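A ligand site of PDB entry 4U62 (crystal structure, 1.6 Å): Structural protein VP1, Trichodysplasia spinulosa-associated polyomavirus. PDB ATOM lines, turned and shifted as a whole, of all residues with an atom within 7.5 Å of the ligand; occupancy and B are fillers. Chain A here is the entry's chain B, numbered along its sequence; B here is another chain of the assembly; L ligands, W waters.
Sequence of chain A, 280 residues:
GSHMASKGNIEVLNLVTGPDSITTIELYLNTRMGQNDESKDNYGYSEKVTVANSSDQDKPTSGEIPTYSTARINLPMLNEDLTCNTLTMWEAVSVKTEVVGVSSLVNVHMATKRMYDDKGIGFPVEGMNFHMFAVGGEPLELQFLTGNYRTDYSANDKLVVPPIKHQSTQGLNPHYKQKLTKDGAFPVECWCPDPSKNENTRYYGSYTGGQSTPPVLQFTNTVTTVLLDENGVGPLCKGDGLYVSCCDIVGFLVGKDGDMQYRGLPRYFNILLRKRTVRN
The backbone carbonyl oxygen of Gln 57 sits close to an oxygen (O9) of the ligand, 3.2 Å away. Residues that only touch the ligand: Thr 61 (3.5 Å), Ala 52 (3.6 Å), His 109 of chain B (3.7 Å), Asn 53 (3.7 Å), Asp 58 (3.8 Å) and Pro 60 (3.9 Å). Hydrophobic or aromatic side chains within 4 Å of the ligand: Ala 52 and His 109 of chain B. Of the 26 residues printed, 11 come within 4 Å of the ligand. The nearest printed residue that does not touch the ligand is Glu 64 (4.7 Å).
Water W1 bridges O4 of the ligand (2.4 Å) and O of Lys 59 (3.1 Å). Water W2 lies within hydrogen-bond range of O of Gln 57 (2.7 Å), N of Asn 53 (2.9 Å) and O9 of the ligand (3.3 Å). Water W3 lies within hydrogen-bond range of O of Val 49 (2.7 Å), NH2 of Arg 114 of chain B (3.1 Å) and O8 of the ligand (3.3 Å).
The backbone carbonyl oxygen (O) of Val 51 sits at hydrogen-bond distance from an oxygen (O6) of the ligand (2.8 Å). NH1 of Arg 114 of chain B sits at hydrogen-bond distance from O8 of the ligand, 2.9 Å away. O4 of the ligand is in hydrogen-bond range of O of Lys 59 (2.5 Å). The backbone NH of Val 51 sits at hydrogen-bond distance from an oxygen (O8) of the ligand (3.1 Å). The backbone NH (N) of Lys 59 is in hydrogen-bond range of an oxygen (O9) of the ligand (3.0 Å). The side-chain hydroxyl (OG1) of Thr 50 is in hydrogen-bond range of a nitrogen (N1) of the ligand, 2.8 Å away.
The guanidinium group of Arg 114 of chain B sits at hydrogen-bond distance from the backbone carbonyl oxygen of Lys 119 of chain B (3.4 Å). O of His 109 of chain B lies within hydrogen-bond range of N of Ala 52 (2.9 Å). O of Ala 52 is in hydrogen-bond range of NZ of Lys 256 of chain B (2.9 Å). The side-chain carboxylate (OE1) of Glu 64 lies within hydrogen-bond range of the side-chain hydroxyl (OG1) of Thr 61 (2.8 Å). ND1 of His 109 of chain B lies within hydrogen-bond range of OD1 of Asp 58 (2.8 Å). O of Asp 58 is in hydrogen-bond range of N of Asp 152, 2.9 Å away. The backbone carbonyl oxygen (O) of Gly 120 of chain B sits at hydrogen-bond distance from the guanidinium group (NE) of Arg 114 of chain B (2.9 Å). The guanidinium group (NE) of Arg 114 of chain B sits close to the backbone carbonyl oxygen (O) of Asp 118 of chain B (3.2 Å).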
ATOM      1  N   LYS A  48     -23.054  38.510  24.366  1.00  0.00           N
ATOM      2  CA  LYS A  48     -21.907  37.657  24.030  1.00  0.00           C
ATOM      3  C   LYS A  48     -22.258  36.166  24.160  1.00  0.00           C
ATOM      4  O   LYS A  48     -22.887  35.752  25.145  1.00  0.00           O
ATOM      5  CB  LYS A  48     -20.737  38.016  24.947  1.00  0.00           C
ATOM      6  CG  LYS A  48     -19.496  37.194  24.701  1.00  0.00           C
ATOM      7  N   VAL A  49     -21.882  35.367  23.155  1.00  0.00           N
ATOM      8  CA  VAL A  49     -22.104  33.920  23.181  1.00  0.00           C
ATOM      9  C   VAL A  49     -21.194  33.239  24.215  1.00  0.00           C
ATOM     10  O   VAL A  49     -20.013  33.580  24.358  1.00  0.00           O
ATOM     11  CB  VAL A  49     -21.889  33.307  21.777  1.00  0.00           C
ATOM     12  CG1 VAL A  49     -21.845  31.779  21.813  1.00  0.00           C
ATOM     13  CG2 VAL A  49     -23.002  33.820  20.858  1.00  0.00           C
ATOM     14  N   THR A  50     -21.768  32.291  24.957  1.00  0.00           N
ATOM     15  CA  THR A  50     -21.027  31.478  25.912  1.00  0.00           C
ATOM     16  C   THR A  50     -21.183  30.018  25.527  1.00  0.00           C
ATOM     17  O   THR A  50     -22.094  29.672  24.761  1.00  0.00           O
ATOM     18  CB  THR A  50     -21.508  31.706  27.368  1.00  0.00           C
ATOM     19  OG1 THR A  50     -22.836  31.159  27.560  1.00  0.00           O
ATOM     20  CG2 THR A  50     -21.495  33.197  27.727  1.00  0.00           C
ATOM     21  N   VAL A  51     -20.321  29.159  26.063  1.00  0.00           N
ATOM     22  CA  VAL A  51     -20.268  27.762  25.633  1.00  0.00           C
ATOM     23  C   VAL A  51     -20.339  26.838  26.859  1.00  0.00           C
ATOM     24  O   VAL A  51     -19.593  27.015  27.844  1.00  0.00           O
ATOM     25  CB  VAL A  51     -18.991  27.498  24.808  1.00  0.00           C
ATOM     26  CG1 VAL A  51     -18.819  26.008  24.496  1.00  0.00           C
ATOM     27  CG2 VAL A  51     -19.026  28.332  23.531  1.00  0.00           C
ATOM     28  N   ALA A  52     -21.256  25.882  26.810  1.00  0.00           N
ATOM     29  CA  ALA A  52     -21.465  24.941  27.904  1.00  0.00           C
ATOM     30  C   ALA A  52     -20.227  24.128  28.208  1.00  0.00           C
ATOM     31  O   ALA A  52     -19.485  23.722  27.308  1.00  0.00           O
ATOM     32  CB  ALA A  52     -22.628  24.010  27.609  1.00  0.00           C
ATOM     33  N   ASN A  53     -19.989  23.885  29.490  1.00  0.00           N
ATOM     34  CA  ASN A  53     -18.890  23.018  29.913  1.00  0.00           C
ATOM     35  C   ASN A  53     -19.182  21.537  29.604  1.00  0.00           C
ATOM     36  O   ASN A  53     -18.281  20.767  29.317  1.00  0.00           O
ATOM     37  CB  ASN A  53     -18.608  23.191  31.413  1.00  0.00           C
ATOM     38  CG  ASN A  53     -18.001  24.552  31.753  1.00  0.00           C
ATOM     39  OD1 ASN A  53     -17.402  25.222  30.911  1.00  0.00           O
ATOM     40  ND2 ASN A  53     -18.126  24.945  33.029  1.00  0.00           N
ATOM     41  N   SER A  54     -20.467  21.174  29.683  1.00  0.00           N
ATOM     42  CA  SER A  54     -20.923  19.830  29.352  1.00  0.00           C
ATOM     43  C   SER A  54     -22.398  19.898  28.963  1.00  0.00           C
ATOM     44  O   SER A  54     -23.071  20.895  29.253  1.00  0.00           O
ATOM     45  CB  SER A  54     -20.762  18.904  30.559  1.00  0.00           C
ATOM     46  OG  SER A  54     -21.497  19.405  31.654  1.00  0.00           O
ATOM     47  N   GLN A  57     -24.872  20.801  31.611  1.00  0.00           N
ATOM     48  CA  GLN A  57     -24.724  22.138  32.178  1.00  0.00           C
ATOM     49  C   GLN A  57     -24.766  23.146  31.037  1.00  0.00           C
ATOM     50  O   GLN A  57     -23.891  24.004  30.927  1.00  0.00           O
ATOM     51  CB  GLN A  57     -23.401  22.248  32.948  1.00  0.00           C
ATOM     52  CG  GLN A  57     -23.231  21.190  34.031  1.00  0.00           C
ATOM     53  CD  GLN A  57     -24.292  21.261  35.124  1.00  0.00           C
ATOM     54  OE1 GLN A  57     -24.872  22.314  35.379  1.00  0.00           O
ATOM     55  NE2 GLN A  57     -24.512  20.122  35.792  1.00  0.00           N
ATOM     56  N   ASP A  58     -25.796  23.043  30.213  1.00  0.00           N
ATOM     57  CA  ASP A  58     -25.950  23.900  29.036  1.00  0.00           C
ATOM     58  C   ASP A  58     -27.051  24.905  29.328  1.00  0.00           C
ATOM     59  O   ASP A  58     -28.226  24.619  29.117  1.00  0.00           O
ATOM     60  CB  ASP A  58     -26.270  23.026  27.813  1.00  0.00           C
ATOM     61  CG  ASP A  58     -26.191  23.771  26.484  1.00  0.00           C
ATOM     62  OD1 ASP A  58     -26.140  25.026  26.440  1.00  0.00           O
ATOM     63  OD2 ASP A  58     -26.159  23.051  25.443  1.00  0.00           O
ATOM     64  N   LYS A  59     -26.641  26.058  29.865  1.00  0.00           N
ATOM     65  CA  LYS A  59     -27.550  27.087  30.354  1.00  0.00           C
ATOM     66  C   LYS A  59     -27.164  28.423  29.710  1.00  0.00           C
ATOM     67  O   LYS A  59     -26.316  29.163  30.249  1.00  0.00           O
ATOM     68  CB  LYS A  59     -27.482  27.171  31.871  1.00  0.00           C
ATOM     69  CG  LYS A  59     -28.521  28.086  32.487  1.00  0.00           C
ATOM     70  CD  LYS A  59     -28.404  28.157  34.006  1.00  0.00           C
ATOM     71  CE  LYS A  59     -29.376  29.188  34.549  1.00  0.00           C
ATOM     72  NZ  LYS A  59     -29.404  29.203  36.035  1.00  0.00           N
ATOM     73  N   PRO A  60     -27.771  28.743  28.567  1.00  0.00           N
ATOM     74  CA  PRO A  60     -27.410  30.012  27.915  1.00  0.00           C
ATOM     75  C   PRO A  60     -27.671  31.207  28.823  1.00  0.00           C
ATOM     76  O   PRO A  60     -28.633  31.214  29.583  1.00  0.00           O
ATOM     77  CB  PRO A  60     -28.304  30.066  26.682  1.00  0.00           C
ATOM     78  CG  PRO A  60     -29.188  28.890  26.728  1.00  0.00           C
ATOM     79  CD  PRO A  60     -28.662  27.933  27.727  1.00  0.00           C
ATOM     80  N   THR A  61     -26.798  32.196  28.755  1.00  0.00           N
ATOM     81  CA  THR A  61     -27.017  33.438  29.494  1.00  0.00           C
ATOM     82  C   THR A  61     -28.231  34.195  28.913  1.00  0.00           C
ATOM     83  O   THR A  61     -28.652  34.000  27.740  1.00  0.00           O
ATOM     84  CB  THR A  61     -25.789  34.357  29.464  1.00  0.00           C
ATOM     85  OG1 THR A  61     -25.502  34.727  28.115  1.00  0.00           O
ATOM     86  CG2 THR A  61     -24.559  33.679  30.069  1.00  0.00           C
ATOM     87  N   SER A  62     -28.797  35.079  29.726  1.00  0.00           N
ATOM     88  CA  SER A  62     -29.898  35.886  29.276  1.00  0.00           C
ATOM     89  C   SER A  62     -29.460  36.819  28.151  1.00  0.00           C
ATOM     90  O   SER A  62     -28.481  37.557  28.272  1.00  0.00           O
ATOM     91  CB  SER A  62     -30.480  36.682  30.457  1.00  0.00           C
ATOM     92  OG  SER A  62     -31.601  37.432  30.023  1.00  0.00           O
ATOM     93  N   GLU A  64     -28.444  35.883  25.028  1.00  0.00           N
ATOM     94  CA  GLU A  64     -27.543  35.364  23.996  1.00  0.00           C
ATOM     95  C   GLU A  64     -28.233  34.500  22.921  1.00  0.00           C
ATOM     96  O   GLU A  64     -27.536  34.014  22.022  1.00  0.00           O
ATOM     97  CB  GLU A  64     -26.346  34.637  24.600  1.00  0.00           C
ATOM     98  CG  GLU A  64     -26.603  33.242  25.150  1.00  0.00           C
ATOM     99  CD  GLU A  64     -25.308  32.508  25.434  1.00  0.00           C
ATOM    100  OE1 GLU A  64     -24.890  32.448  26.616  1.00  0.00           O
ATOM    101  OE2 GLU A  64     -24.694  31.996  24.465  1.00  0.00           O
ATOM    102  N   THR A 151     -30.945  21.485  27.359  1.00  0.00           N
ATOM    103  CA  THR A 151     -30.753  22.940  27.393  1.00  0.00           C
ATOM    104  C   THR A 151     -31.675  23.561  28.446  1.00  0.00           C
ATOM    105  O   THR A 151     -32.868  23.297  28.455  1.00  0.00           O
ATOM    106  CB  THR A 151     -30.998  23.571  26.033  1.00  0.00           C
ATOM    107  OG1 THR A 151     -30.272  22.857  25.042  1.00  0.00           O
ATOM    108  CG2 THR A 151     -30.526  25.034  26.031  1.00  0.00           C
ATOM    109  N   ASP A 152     -31.079  24.384  29.309  1.00  0.00           N
ATOM    110  CA  ASP A 152     -31.754  25.019  30.444  1.00  0.00           C
ATOM    111  C   ASP A 152     -31.972  26.492  30.102  1.00  0.00           C
ATOM    112  O   ASP A 152     -31.014  27.246  30.003  1.00  0.00           O
ATOM    113  CB  ASP A 152     -30.815  24.867  31.655  1.00  0.00           C
ATOM    114  CG  ASP A 152     -31.325  25.535  32.901  1.00  0.00           C
ATOM    115  OD1 ASP A 152     -32.365  26.208  32.869  1.00  0.00           O
ATOM    116  OD2 ASP A 152     -30.660  25.355  33.947  1.00  0.00           O
ATOM    117  N   ALA A 155     -32.233  31.068  32.706  1.00  0.00           N
ATOM    118  CA  ALA A 155     -31.643  32.401  32.879  1.00  0.00           C
ATOM    119  C   ALA A 155     -32.580  33.506  32.358  1.00  0.00           C
ATOM    120  O   ALA A 155     -32.431  34.663  32.728  1.00  0.00           O
ATOM    121  CB  ALA A 155     -30.287  32.484  32.190  1.00  0.00           C
ATOM    122  N   VAL B 108     -24.844  27.681  18.992  1.00  0.00           N
ATOM    123  CA  VAL B 108     -23.398  27.697  19.132  1.00  0.00           C
ATOM    124  C   VAL B 108     -22.990  27.810  20.596  1.00  0.00           C
ATOM    125  O   VAL B 108     -21.884  28.258  20.909  1.00  0.00           O
ATOM    126  CB  VAL B 108     -22.753  28.839  18.289  1.00  0.00           C
ATOM    127  CG1 VAL B 108     -22.887  28.527  16.816  1.00  0.00           C
ATOM    128  CG2 VAL B 108     -23.390  30.191  18.618  1.00  0.00           C
ATOM    129  N   HIS B 109     -23.874  27.359  21.496  1.00  0.00           N
ATOM    130  CA  HIS B 109     -23.535  27.334  22.930  1.00  0.00           C
ATOM    131  C   HIS B 109     -23.468  25.932  23.504  1.00  0.00           C
ATOM    132  O   HIS B 109     -23.317  25.789  24.745  1.00  0.00           O
ATOM    133  CB  HIS B 109     -24.496  28.206  23.771  1.00  0.00           C
ATOM    134  CG  HIS B 109     -25.930  27.819  23.611  1.00  0.00           C
ATOM    135  ND1 HIS B 109     -26.496  26.717  24.231  1.00  0.00           N
ATOM    136  CD2 HIS B 109     -26.915  28.389  22.890  1.00  0.00           C
ATOM    137  CE1 HIS B 109     -27.759  26.633  23.883  1.00  0.00           C
ATOM    138  NE2 HIS B 109     -28.047  27.638  23.064  1.00  0.00           N
ATOM    139  N   MET B 110     -23.578  24.904  22.661  1.00  0.00           N
ATOM    140  CA  MET B 110     -23.457  23.522  23.154  1.00  0.00           C
ATOM    141  C   MET B 110     -22.011  23.233  23.535  1.00  0.00           C
ATOM    142  O   MET B 110     -21.092  23.962  23.177  1.00  0.00           O
ATOM    143  CB  MET B 110     -23.929  22.523  22.110  1.00  0.00           C
ATOM    144  CG  MET B 110     -25.428  22.592  21.879  1.00  0.00           C
ATOM    145  SD  MET B 110     -26.037  21.346  20.739  1.00  0.00           S
ATOM    146  CE  MET B 110     -25.254  21.886  19.236  1.00  0.00           C
ATOM    147  N   ALA B 111     -21.805  22.145  24.285  1.00  0.00           N
ATOM    148  CA  ALA B 111     -20.485  21.740  24.769  1.00  0.00           C
ATOM    149  C   ALA B 111     -19.639  21.222  23.622  1.00  0.00           C
ATOM    150  O   ALA B 111     -19.675  20.035  23.284  1.00  0.00           O
ATOM    151  CB  ALA B 111     -20.640  20.696  25.881  1.00  0.00           C
ATOM    152  N   ARG B 114     -14.472  25.420  20.442  1.00  0.00           N
ATOM    153  CA  ARG B 114     -14.881  26.795  20.155  1.00  0.00           C
ATOM    154  C   ARG B 114     -13.826  27.571  19.403  1.00  0.00           C
ATOM    155  O   ARG B 114     -12.643  27.201  19.359  1.00  0.00           O
ATOM    156  CB  ARG B 114     -15.364  27.528  21.428  1.00  0.00           C
ATOM    157  CG  ARG B 114     -14.343  27.693  22.507  1.00  0.00           C
ATOM    158  CD  ARG B 114     -14.981  28.116  23.839  1.00  0.00           C
ATOM    159  NE  ARG B 114     -15.710  29.382  23.726  1.00  0.00           N
ATOM    160  CZ  ARG B 114     -16.266  30.041  24.739  1.00  0.00           C
ATOM    161  NH1 ARG B 114     -16.195  29.581  25.983  1.00  0.00           N
ATOM    162  NH2 ARG B 114     -16.900  31.180  24.518  1.00  0.00           N
ATOM    163  N   ASP B 118     -10.585  29.914  22.821  1.00  0.00           N
ATOM    164  CA  ASP B 118     -11.626  29.665  23.843  1.00  0.00           C
ATOM    165  C   ASP B 118     -12.532  30.839  24.190  1.00  0.00           C
ATOM    166  O   ASP B 118     -13.234  30.813  25.211  1.00  0.00           O
ATOM    167  CB  ASP B 118     -11.006  29.067  25.114  1.00  0.00           C
ATOM    168  CG  ASP B 118     -10.580  27.620  24.941  1.00  0.00           C
ATOM    169  OD1 ASP B 118     -11.232  26.893  24.152  1.00  0.00           O
ATOM    170  OD2 ASP B 118      -9.599  27.221  25.582  1.00  0.00           O
ATOM    171  N   LYS B 119     -12.567  31.865  23.320  1.00  0.00           N
ATOM    172  CA  LYS B 119     -13.364  33.051  23.560  1.00  0.00           C
ATOM    173  C   LYS B 119     -14.579  33.182  22.665  1.00  0.00           C
ATOM    174  O   LYS B 119     -15.523  33.863  23.021  1.00  0.00           O
ATOM    175  CB  LYS B 119     -12.511  34.308  23.428  1.00  0.00           C
ATOM    176  CG  LYS B 119     -11.369  34.366  24.430  1.00  0.00           C
ATOM    177  CD  LYS B 119     -11.867  34.620  25.837  1.00  0.00           C
ATOM    178  CE  LYS B 119     -10.708  34.854  26.800  1.00  0.00           C
ATOM    179  NZ  LYS B 119      -9.818  33.662  26.883  1.00  0.00           N
ATOM    180  N   GLY B 120     -14.547  32.530  21.511  1.00  0.00           N
ATOM    181  CA  GLY B 120     -15.611  32.700  20.517  1.00  0.00           C
ATOM    182  C   GLY B 120     -16.721  31.663  20.596  1.00  0.00           C
ATOM    183  O   GLY B 120     -16.888  30.959  21.606  1.00  0.00           O
ATOM    184  N   LYS B 256     -15.629  18.966  22.765  1.00  0.00           N
ATOM    185  CA  LYS B 256     -14.530  19.717  23.363  1.00  0.00           C
ATOM    186  C   LYS B 256     -13.147  19.207  22.989  1.00  0.00           C
ATOM    187  O   LYS B 256     -12.237  19.992  22.727  1.00  0.00           O
ATOM    188  CB  LYS B 256     -14.640  19.660  24.905  1.00  0.00           C
ATOM    189  CG  LYS B 256     -15.904  20.307  25.464  1.00  0.00           C
ATOM    190  CD  LYS B 256     -15.622  21.665  26.083  1.00  0.00           C
ATOM    191  CE  LYS B 256     -16.911  22.427  26.386  1.00  0.00           C
ATOM    192  NZ  LYS B 256     -16.606  23.791  26.899  1.00  0.00           N
HETATM  193  C1  LIG L   1     -21.357  32.480  32.481  1.00  0.00           C
HETATM  194  C2  LIG L   1     -21.348  31.054  33.000  1.00  0.00           C
HETATM  195  C3  LIG L   1     -22.769  30.498  33.101  1.00  0.00           C
HETATM  196  C4  LIG L   1     -23.368  30.172  31.740  1.00  0.00           C
HETATM  197  C5  LIG L   1     -22.451  29.311  30.873  1.00  0.00           C
HETATM  198  C6  LIG L   1     -21.076  29.996  30.827  1.00  0.00           C
HETATM  199  C7  LIG L   1     -20.024  29.245  30.002  1.00  0.00           C
HETATM  200  C8  LIG L   1     -18.654  29.945  30.087  1.00  0.00           C
HETATM  201  C9  LIG L   1     -17.797  29.704  28.846  1.00  0.00           C
HETATM  202  C10 LIG L   1     -23.607  27.970  29.139  1.00  0.00           C
HETATM  203  C11 LIG L   1     -24.066  27.897  27.694  1.00  0.00           C
HETATM  204  N1  LIG L   1     -23.001  29.112  29.535  1.00  0.00           N
HETATM  205  O1  LIG L   1     -22.344  33.220  32.684  1.00  0.00           O
HETATM  206  O2  LIG L   1     -20.343  32.886  31.874  1.00  0.00           O
HETATM  207  O3  LIG L   1     -20.815  31.005  34.331  1.00  0.00           O
HETATM  208  O4  LIG L   1     -24.594  29.490  32.026  1.00  0.00           O
HETATM  209  O5  LIG L   1     -20.569  30.181  32.159  1.00  0.00           O
HETATM  210  O6  LIG L   1     -19.925  27.898  30.436  1.00  0.00           O
HETATM  211  O7  LIG L   1     -18.835  31.354  30.207  1.00  0.00           O
HETATM  212  O8  LIG L   1     -18.229  30.596  27.806  1.00  0.00           O
HETATM  213  O9  LIG L   1     -23.783  27.015  29.885  1.00  0.00           O
HETATM  214  O   HOH W   1     -26.396  30.889  32.772  1.00  0.00           O
HETATM  215  O   HOH W   2     -21.586  25.193  31.535  1.00  0.00           O
HETATM  216  O   HOH W   3     -18.070  33.536  26.238  1.00  0.00           O
